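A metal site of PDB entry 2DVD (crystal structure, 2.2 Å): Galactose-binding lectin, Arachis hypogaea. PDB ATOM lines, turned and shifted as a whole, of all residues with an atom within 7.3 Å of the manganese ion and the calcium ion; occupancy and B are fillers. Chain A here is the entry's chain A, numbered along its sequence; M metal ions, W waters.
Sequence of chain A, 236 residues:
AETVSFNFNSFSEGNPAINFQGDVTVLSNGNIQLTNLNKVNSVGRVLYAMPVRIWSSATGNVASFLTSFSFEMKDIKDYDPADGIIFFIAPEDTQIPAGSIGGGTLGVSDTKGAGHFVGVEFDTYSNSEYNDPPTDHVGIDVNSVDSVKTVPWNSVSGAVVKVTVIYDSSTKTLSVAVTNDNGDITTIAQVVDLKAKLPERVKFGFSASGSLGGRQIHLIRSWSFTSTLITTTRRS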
ATOM      1  N   ASP A  83      33.174 -20.159  -7.755  1.00  0.00           N
ATOM      2  CA  ASP A  83      32.139 -21.115  -7.353  1.00  0.00           C
ATOM      3  C   ASP A  83      31.103 -20.551  -6.379  1.00  0.00           C
ATOM      4  O   ASP A  83      30.060 -21.168  -6.172  1.00  0.00           O
ATOM      5  CB  ASP A  83      32.791 -22.346  -6.718  1.00  0.00           C
ATOM      6  CG  ASP A  83      33.241 -23.353  -7.754  1.00  0.00           C
ATOM      7  OD1 ASP A  83      32.421 -24.241  -8.101  1.00  0.00           O
ATOM      8  OD2 ASP A  83      34.387 -23.258  -8.240  1.00  0.00           O
ATOM      9  N   GLY A  84      31.390 -19.408  -5.768  1.00  0.00           N
ATOM     10  CA  GLY A  84      30.433 -18.832  -4.836  1.00  0.00           C
ATOM     11  C   GLY A  84      31.021 -18.430  -3.497  1.00  0.00           C
ATOM     12  O   GLY A  84      32.209 -18.623  -3.244  1.00  0.00           O
ATOM     13  N   GLY A 103      37.060 -24.868  -5.640  1.00  0.00           N
ATOM     14  CA  GLY A 103      35.869 -25.192  -6.399  1.00  0.00           C
ATOM     15  C   GLY A 103      34.603 -25.329  -5.590  1.00  0.00           C
ATOM     16  O   GLY A 103      34.264 -24.460  -4.780  1.00  0.00           O
ATOM     17  N   GLY A 104      33.888 -26.438  -5.804  1.00  0.00           N
ATOM     18  CA  GLY A 104      32.640 -26.678  -5.094  1.00  0.00           C
ATOM     19  C   GLY A 104      32.732 -26.812  -3.586  1.00  0.00           C
ATOM     20  O   GLY A 104      31.705 -26.773  -2.905  1.00  0.00           O
ATOM     21  N   THR A 105      33.935 -26.981  -3.057  1.00  0.00           N
ATOM     22  CA  THR A 105      34.106 -27.108  -1.613  1.00  0.00           C
ATOM     23  C   THR A 105      33.938 -25.757  -0.905  1.00  0.00           C
ATOM     24  O   THR A 105      33.842 -25.695   0.315  1.00  0.00           O
ATOM     25  CB  THR A 105      35.515 -27.624  -1.248  1.00  0.00           C
ATOM     26  OG1 THR A 105      36.489 -26.621  -1.566  1.00  0.00           O
ATOM     27  CG2 THR A 105      35.829 -28.892  -2.026  1.00  0.00           C
ATOM     28  N   LEU A 106      33.914 -24.683  -1.698  1.00  0.00           N
ATOM     29  CA  LEU A 106      33.758 -23.319  -1.186  1.00  0.00           C
ATOM     30  C   LEU A 106      34.822 -22.937  -0.163  1.00  0.00           C
ATOM     31  O   LEU A 106      34.678 -21.944   0.558  1.00  0.00           O
ATOM     32  CB  LEU A 106      32.369 -23.136  -0.583  1.00  0.00           C
ATOM     33  CG  LEU A 106      31.200 -23.372  -1.558  1.00  0.00           C
ATOM     34  CD1 LEU A 106      29.877 -23.043  -0.868  1.00  0.00           C
ATOM     35  CD2 LEU A 106      31.399 -22.515  -2.795  1.00  0.00           C
ATOM     36  N   GLU A 121      25.403 -20.672   2.160  1.00  0.00           N
ATOM     37  CA  GLU A 121      26.116 -20.533   0.900  1.00  0.00           C
ATOM     38  C   GLU A 121      25.331 -19.859  -0.209  1.00  0.00           C
ATOM     39  O   GLU A 121      24.099 -19.962  -0.299  1.00  0.00           O
ATOM     40  CB  GLU A 121      26.593 -21.918   0.426  1.00  0.00           C
ATOM     41  CG  GLU A 121      25.474 -22.903   0.214  1.00  0.00           C
ATOM     42  CD  GLU A 121      25.892 -24.099  -0.615  1.00  0.00           C
ATOM     43  OE1 GLU A 121      26.788 -24.852  -0.173  1.00  0.00           O
ATOM     44  OE2 GLU A 121      25.331 -24.279  -1.705  1.00  0.00           O
ATOM     45  N   PHE A 122      26.070 -19.155  -1.050  1.00  0.00           N
ATOM     46  CA  PHE A 122      25.559 -18.432  -2.197  1.00  0.00           C
ATOM     47  C   PHE A 122      26.350 -19.064  -3.334  1.00  0.00           C
ATOM     48  O   PHE A 122      27.403 -18.577  -3.734  1.00  0.00           O
ATOM     49  CB  PHE A 122      25.857 -16.949  -2.022  1.00  0.00           C
ATOM     50  CG  PHE A 122      25.250 -16.383  -0.763  1.00  0.00           C
ATOM     51  CD1 PHE A 122      23.924 -15.971  -0.743  1.00  0.00           C
ATOM     52  CD2 PHE A 122      25.984 -16.333   0.417  1.00  0.00           C
ATOM     53  CE1 PHE A 122      23.329 -15.516   0.444  1.00  0.00           C
ATOM     54  CE2 PHE A 122      25.410 -15.879   1.609  1.00  0.00           C
ATOM     55  CZ  PHE A 122      24.081 -15.473   1.617  1.00  0.00           C
ATOM     56  N   ASP A 123      25.819 -20.187  -3.784  1.00  0.00           N
ATOM     57  CA  ASP A 123      26.387 -21.048  -4.803  1.00  0.00           C
ATOM     58  C   ASP A 123      26.051 -20.665  -6.237  1.00  0.00           C
ATOM     59  O   ASP A 123      24.884 -20.551  -6.592  1.00  0.00           O
ATOM     60  CB  ASP A 123      25.897 -22.462  -4.537  1.00  0.00           C
ATOM     61  CG  ASP A 123      26.833 -23.497  -5.026  1.00  0.00           C
ATOM     62  OD1 ASP A 123      27.399 -23.307  -6.127  1.00  0.00           O
ATOM     63  OD2 ASP A 123      27.003 -24.508  -4.319  1.00  0.00           O
ATOM     64  N   THR A 124      27.070 -20.517  -7.070  1.00  0.00           N
ATOM     65  CA  THR A 124      26.853 -20.121  -8.461  1.00  0.00           C
ATOM     66  C   THR A 124      27.246 -21.168  -9.499  1.00  0.00           C
ATOM     67  O   THR A 124      27.366 -20.862 -10.675  1.00  0.00           O
ATOM     68  CB  THR A 124      27.619 -18.819  -8.789  1.00  0.00           C
ATOM     69  OG1 THR A 124      29.015 -19.100  -8.894  1.00  0.00           O
ATOM     70  CG2 THR A 124      27.407 -17.790  -7.680  1.00  0.00           C
ATOM     71  N   TYR A 125      27.470 -22.403  -9.054  1.00  0.00           N
ATOM     72  CA  TYR A 125      27.843 -23.471  -9.986  1.00  0.00           C
ATOM     73  C   TYR A 125      27.301 -24.804  -9.496  1.00  0.00           C
ATOM     74  O   TYR A 125      27.415 -25.128  -8.323  1.00  0.00           O
ATOM     75  CB  TYR A 125      29.363 -23.563 -10.127  1.00  0.00           C
ATOM     76  CG  TYR A 125      29.778 -24.591 -11.155  1.00  0.00           C
ATOM     77  CD1 TYR A 125      29.852 -25.941 -10.820  1.00  0.00           C
ATOM     78  CD2 TYR A 125      30.025 -24.223 -12.474  1.00  0.00           C
ATOM     79  CE1 TYR A 125      30.148 -26.905 -11.785  1.00  0.00           C
ATOM     80  CE2 TYR A 125      30.319 -25.171 -13.445  1.00  0.00           C
ATOM     81  CZ  TYR A 125      30.376 -26.509 -13.089  1.00  0.00           C
ATOM     82  OH  TYR A 125      30.650 -27.450 -14.053  1.00  0.00           O
ATOM     83  N   SER A 126      26.703 -25.585 -10.400  1.00  0.00           N
ATOM     84  CA  SER A 126      26.133 -26.859  -9.986  1.00  0.00           C
ATOM     85  C   SER A 126      27.114 -28.040  -9.941  1.00  0.00           C
ATOM     86  O   SER A 126      27.489 -28.596 -10.975  1.00  0.00           O
ATOM     87  CB  SER A 126      24.950 -27.209 -10.900  1.00  0.00           C
ATOM     88  OG  SER A 126      24.236 -28.319 -10.400  1.00  0.00           O
ATOM     89  N   ASN A 127      27.517 -28.418  -8.724  1.00  0.00           N
ATOM     90  CA  ASN A 127      28.420 -29.552  -8.514  1.00  0.00           C
ATOM     91  C   ASN A 127      27.573 -30.777  -8.206  1.00  0.00           C
ATOM     92  O   ASN A 127      27.029 -30.907  -7.105  1.00  0.00           O
ATOM     93  CB  ASN A 127      29.349 -29.301  -7.316  1.00  0.00           C
ATOM     94  CG  ASN A 127      30.387 -28.241  -7.592  1.00  0.00           C
ATOM     95  OD1 ASN A 127      30.082 -27.069  -7.627  1.00  0.00           O
ATOM     96  ND2 ASN A 127      31.635 -28.675  -7.808  1.00  0.00           N
ATOM     97  N   SER A 128      27.453 -31.681  -9.178  1.00  0.00           N
ATOM     98  CA  SER A 128      26.661 -32.888  -8.990  1.00  0.00           C
ATOM     99  C   SER A 128      27.237 -33.763  -7.881  1.00  0.00           C
ATOM    100  O   SER A 128      26.495 -34.408  -7.152  1.00  0.00           O
ATOM    101  CB  SER A 128      26.588 -33.696 -10.287  1.00  0.00           C
ATOM    102  OG  SER A 128      27.872 -34.098 -10.720  1.00  0.00           O
ATOM    103  N   GLU A 129      28.555 -33.765  -7.736  1.00  0.00           N
ATOM    104  CA  GLU A 129      29.185 -34.578  -6.703  1.00  0.00           C
ATOM    105  C   GLU A 129      28.752 -34.153  -5.304  1.00  0.00           C
ATOM    106  O   GLU A 129      29.016 -34.864  -4.330  1.00  0.00           O
ATOM    107  CB  GLU A 129      30.720 -34.538  -6.804  1.00  0.00           C
ATOM    108  CG  GLU A 129      31.340 -33.196  -6.473  1.00  0.00           C
ATOM    109  CD  GLU A 129      31.468 -32.278  -7.678  1.00  0.00           C
ATOM    110  OE1 GLU A 129      30.583 -32.329  -8.565  1.00  0.00           O
ATOM    111  OE2 GLU A 129      32.440 -31.503  -7.731  1.00  0.00           O
ATOM    112  N   TYR A 130      28.093 -32.993  -5.193  1.00  0.00           N
ATOM    113  CA  TYR A 130      27.616 -32.499  -3.902  1.00  0.00           C
ATOM    114  C   TYR A 130      26.097 -32.323  -3.908  1.00  0.00           C
ATOM    115  O   TYR A 130      25.540 -31.629  -3.060  1.00  0.00           O
ATOM    116  CB  TYR A 130      28.275 -31.166  -3.543  1.00  0.00           C
ATOM    117  CG  TYR A 130      29.787 -31.207  -3.501  1.00  0.00           C
ATOM    118  CD1 TYR A 130      30.452 -32.252  -2.865  1.00  0.00           C
ATOM    119  CD2 TYR A 130      30.541 -30.201  -4.095  1.00  0.00           C
ATOM    120  CE1 TYR A 130      31.851 -32.291  -2.828  1.00  0.00           C
ATOM    121  CE2 TYR A 130      31.924 -30.227  -4.069  1.00  0.00           C
ATOM    122  CZ  TYR A 130      32.579 -31.270  -3.424  1.00  0.00           C
ATOM    123  OH  TYR A 130      33.951 -31.296  -3.412  1.00  0.00           O
ATOM    124  N   ASN A 131      25.454 -32.952  -4.887  1.00  0.00           N
ATOM    125  CA  ASN A 131      24.004 -32.899  -5.039  1.00  0.00           C
ATOM    126  C   ASN A 131      23.408 -31.494  -5.111  1.00  0.00           C
ATOM    127  O   ASN A 131      22.344 -31.234  -4.537  1.00  0.00           O
ATOM    128  CB  ASN A 131      23.331 -33.692  -3.919  1.00  0.00           C
ATOM    129  CG  ASN A 131      23.665 -35.167  -3.983  1.00  0.00           C
ATOM    130  OD1 ASN A 131      23.471 -35.826  -5.012  1.00  0.00           O
ATOM    131  ND2 ASN A 131      24.158 -35.706  -2.875  1.00  0.00           N
ATOM    132  N   ASP A 132      24.091 -30.583  -5.791  1.00  0.00           N
ATOM    133  CA  ASP A 132      23.576 -29.229  -5.932  1.00  0.00           C
ATOM    134  C   ASP A 132      22.363 -29.208  -6.824  1.00  0.00           C
ATOM    135  O   ASP A 132      22.224 -30.034  -7.726  1.00  0.00           O
ATOM    136  CB  ASP A 132      24.604 -28.299  -6.588  1.00  0.00           C
ATOM    137  CG  ASP A 132      25.677 -27.854  -5.642  1.00  0.00           C
ATOM    138  OD1 ASP A 132      25.345 -27.527  -4.491  1.00  0.00           O
ATOM    139  OD2 ASP A 132      26.846 -27.810  -6.063  1.00  0.00           O
ATOM    140  N   PRO A 133      21.440 -28.266  -6.570  1.00  0.00           N
ATOM    141  CA  PRO A 133      20.265 -28.216  -7.435  1.00  0.00           C
ATOM    142  C   PRO A 133      20.809 -27.740  -8.791  1.00  0.00           C
ATOM    143  O   PRO A 133      21.943 -27.291  -8.884  1.00  0.00           O
ATOM    144  CB  PRO A 133      19.368 -27.184  -6.724  1.00  0.00           C
ATOM    145  CG  PRO A 133      20.346 -26.329  -5.974  1.00  0.00           C
ATOM    146  CD  PRO A 133      21.322 -27.331  -5.444  1.00  0.00           C
ATOM    147  N   THR A 135      20.269 -25.001 -10.662  1.00  0.00           N
ATOM    148  CA  THR A 135      20.593 -23.583 -10.861  1.00  0.00           C
ATOM    149  C   THR A 135      21.195 -22.931  -9.619  1.00  0.00           C
ATOM    150  O   THR A 135      21.275 -23.549  -8.568  1.00  0.00           O
ATOM    151  CB  THR A 135      19.346 -22.772 -11.276  1.00  0.00           C
ATOM    152  OG1 THR A 135      18.480 -22.594 -10.145  1.00  0.00           O
ATOM    153  CG2 THR A 135      18.582 -23.488 -12.383  1.00  0.00           C
ATOM    154  N   HIS A 137      21.802 -20.990  -6.238  1.00  0.00           N
ATOM    155  CA  HIS A 137      20.984 -21.183  -5.061  1.00  0.00           C
ATOM    156  C   HIS A 137      21.641 -20.728  -3.765  1.00  0.00           C
ATOM    157  O   HIS A 137      22.861 -20.588  -3.689  1.00  0.00           O
ATOM    158  CB  HIS A 137      20.653 -22.663  -4.934  1.00  0.00           C
ATOM    159  CG  HIS A 137      21.862 -23.537  -4.940  1.00  0.00           C
ATOM    160  ND1 HIS A 137      22.607 -23.766  -6.083  1.00  0.00           N
ATOM    161  CD2 HIS A 137      22.507 -24.186  -3.944  1.00  0.00           C
ATOM    162  CE1 HIS A 137      23.648 -24.529  -5.779  1.00  0.00           C
ATOM    163  NE2 HIS A 137      23.603 -24.790  -4.488  1.00  0.00           N
ATOM    164  N   VAL A 138      20.806 -20.513  -2.765  1.00  0.00           N
ATOM    165  CA  VAL A 138      21.272 -20.145  -1.443  1.00  0.00           C
ATOM    166  C   VAL A 138      21.038 -21.447  -0.668  1.00  0.00           C
ATOM    167  O   VAL A 138      20.006 -22.097  -0.841  1.00  0.00           O
ATOM    168  CB  VAL A 138      20.430 -19.014  -0.840  1.00  0.00           C
ATOM    169  CG1 VAL A 138      20.923 -18.687   0.573  1.00  0.00           C
ATOM    170  CG2 VAL A 138      20.530 -17.778  -1.719  1.00  0.00           C
ATOM    171  N   GLY A 139      21.988 -21.833   0.166  1.00  0.00           N
ATOM    172  CA  GLY A 139      21.816 -23.072   0.909  1.00  0.00           C
ATOM    173  C   GLY A 139      22.241 -22.998   2.353  1.00  0.00           C
ATOM    174  O   GLY A 139      23.066 -22.177   2.736  1.00  0.00           O
ATOM    175  N   ASP A 141      24.094 -25.043   5.126  1.00  0.00           N
ATOM    176  CA  ASP A 141      24.990 -26.178   5.259  1.00  0.00           C
ATOM    177  C   ASP A 141      25.363 -26.497   6.698  1.00  0.00           C
ATOM    178  O   ASP A 141      25.558 -25.606   7.515  1.00  0.00           O
ATOM    179  CB  ASP A 141      26.289 -25.921   4.470  1.00  0.00           C
ATOM    180  CG  ASP A 141      26.041 -25.589   3.012  1.00  0.00           C
ATOM    181  OD1 ASP A 141      24.920 -25.836   2.504  1.00  0.00           O
ATOM    182  OD2 ASP A 141      26.983 -25.087   2.365  1.00  0.00           O
ATOM    183  N   VAL A 145      28.900 -29.375   2.165  1.00  0.00           N
ATOM    184  CA  VAL A 145      28.444 -28.511   1.071  1.00  0.00           C
ATOM    185  C   VAL A 145      27.291 -29.185   0.351  1.00  0.00           C
ATOM    186  O   VAL A 145      26.739 -28.649  -0.612  1.00  0.00           O
ATOM    187  CB  VAL A 145      29.583 -28.157   0.079  1.00  0.00           C
ATOM    188  CG1 VAL A 145      30.537 -27.154   0.736  1.00  0.00           C
ATOM    189  CG2 VAL A 145      30.329 -29.409  -0.336  1.00  0.00           C
ATOM    190  N   ASP A 146      26.924 -30.381   0.804  1.00  0.00           N
ATOM    191  CA  ASP A 146      25.775 -31.066   0.253  1.00  0.00           C
ATOM    192  C   ASP A 146      24.715 -30.487   1.193  1.00  0.00           C
ATOM    193  O   ASP A 146      24.415 -31.043   2.245  1.00  0.00           O
ATOM    194  CB  ASP A 146      25.870 -32.581   0.429  1.00  0.00           C
ATOM    195  CG  ASP A 146      24.718 -33.327  -0.236  1.00  0.00           C
ATOM    196  OD1 ASP A 146      23.587 -32.814  -0.194  1.00  0.00           O
ATOM    197  OD2 ASP A 146      24.936 -34.411  -0.805  1.00  0.00           O
ATOM    198  N   SER A 147      24.188 -29.327   0.803  1.00  0.00           N
ATOM    199  CA  SER A 147      23.218 -28.610   1.612  1.00  0.00           C
ATOM    200  C   SER A 147      22.075 -29.404   2.235  1.00  0.00           C
ATOM    201  O   SER A 147      21.468 -30.282   1.611  1.00  0.00           O
ATOM    202  CB  SER A 147      22.627 -27.460   0.799  1.00  0.00           C
ATOM    203  OG  SER A 147      23.645 -26.550   0.412  1.00  0.00           O
ATOM    204  N   THR A 150      18.165 -26.045   0.229  1.00  0.00           N
ATOM    205  CA  THR A 150      18.500 -24.993  -0.719  1.00  0.00           C
ATOM    206  C   THR A 150      17.234 -24.332  -1.243  1.00  0.00           C
ATOM    207  O   THR A 150      16.136 -24.850  -1.086  1.00  0.00           O
ATOM    208  CB  THR A 150      19.278 -25.519  -1.946  1.00  0.00           C
ATOM    209  OG1 THR A 150      18.388 -26.258  -2.802  1.00  0.00           O
ATOM    210  CG2 THR A 150      20.429 -26.415  -1.525  1.00  0.00           C
HETATM  211 MN    MN M   1      25.492 -25.808  -3.328  1.00  0.00          MN
HETATM  212 CA    CA M   2      28.449 -25.720  -6.120  1.00  0.00          CA
HETATM  213  O   HOH W   1      23.928 -26.995  -2.158  1.00  0.00           O
HETATM  214  O   HOH W   2      27.355 -26.562  -1.951  1.00  0.00           O
HETATM  215  O   HOH W   3      30.122 -23.771  -6.338  1.00  0.00           O
HETATM  216  O   HOH W   4      29.109 -26.489  -3.992  1.00  0.00           O
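OE1 of Glu 121 sits close to OD2 of Asp 141 (2.6 Å). N of Glu 121 lies within hydrogen-bond range of O of Gly 139 (2.8 Å). The backbone carbonyl oxygen (O) of Thr 135 is in hydrogen-bond range of a ring nitrogen (ND1) of His 137, at 2.8 Å. ND2 of Asn 127 lies within hydrogen-bond range of OE2 of Glu 129, 2.9 Å away.
Water W2 bridges OE1 of Glu 121 (2.5 Å) and O of Val 145 (2.6 Å).
Within 4 Å of the manganese ion: Glu 121, Asp 123, Asp 132 and His 137. Along chain A the residues within 4 Å of the manganese ion span positions 121 to 137.
The calcium ion is bound by water W4 (2.4 Å), the backbone carbonyl oxygen (O) of Tyr 125 (2.5 Å), water W3 (2.6 Å), the side-chain amide oxygen (OD1) of Asn 127 (2.6 Å), the side-chain carboxylate (OD2) of Asp 123 (2.6 Å), the side-chain carboxylate (OD1) of Asp 123 (2.6 Å) and the side-chain carboxylate (OD2) of Asp 132 (2.6 Å).
Four residues have an atom within 4 Å of the calcium ion: Asp 123, Tyr 125, Asn 127 and Asp 132. Along chain A the residues within 4 Å of the calcium ion span positions 123 to 132. The nearest printed residue that does not touch the calcium ion is Gly 104 (4.4 Å).
The manganese ion is bound by OD1 of Asp 132 (2.1 Å), OD2 of Asp 123 (2.2 Å), OE2 of Glu 121 (2.2 Å), water W1 (2.3 Å), water W2 (2.4 Å) and NE2 of His 137 (2.4 Å).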
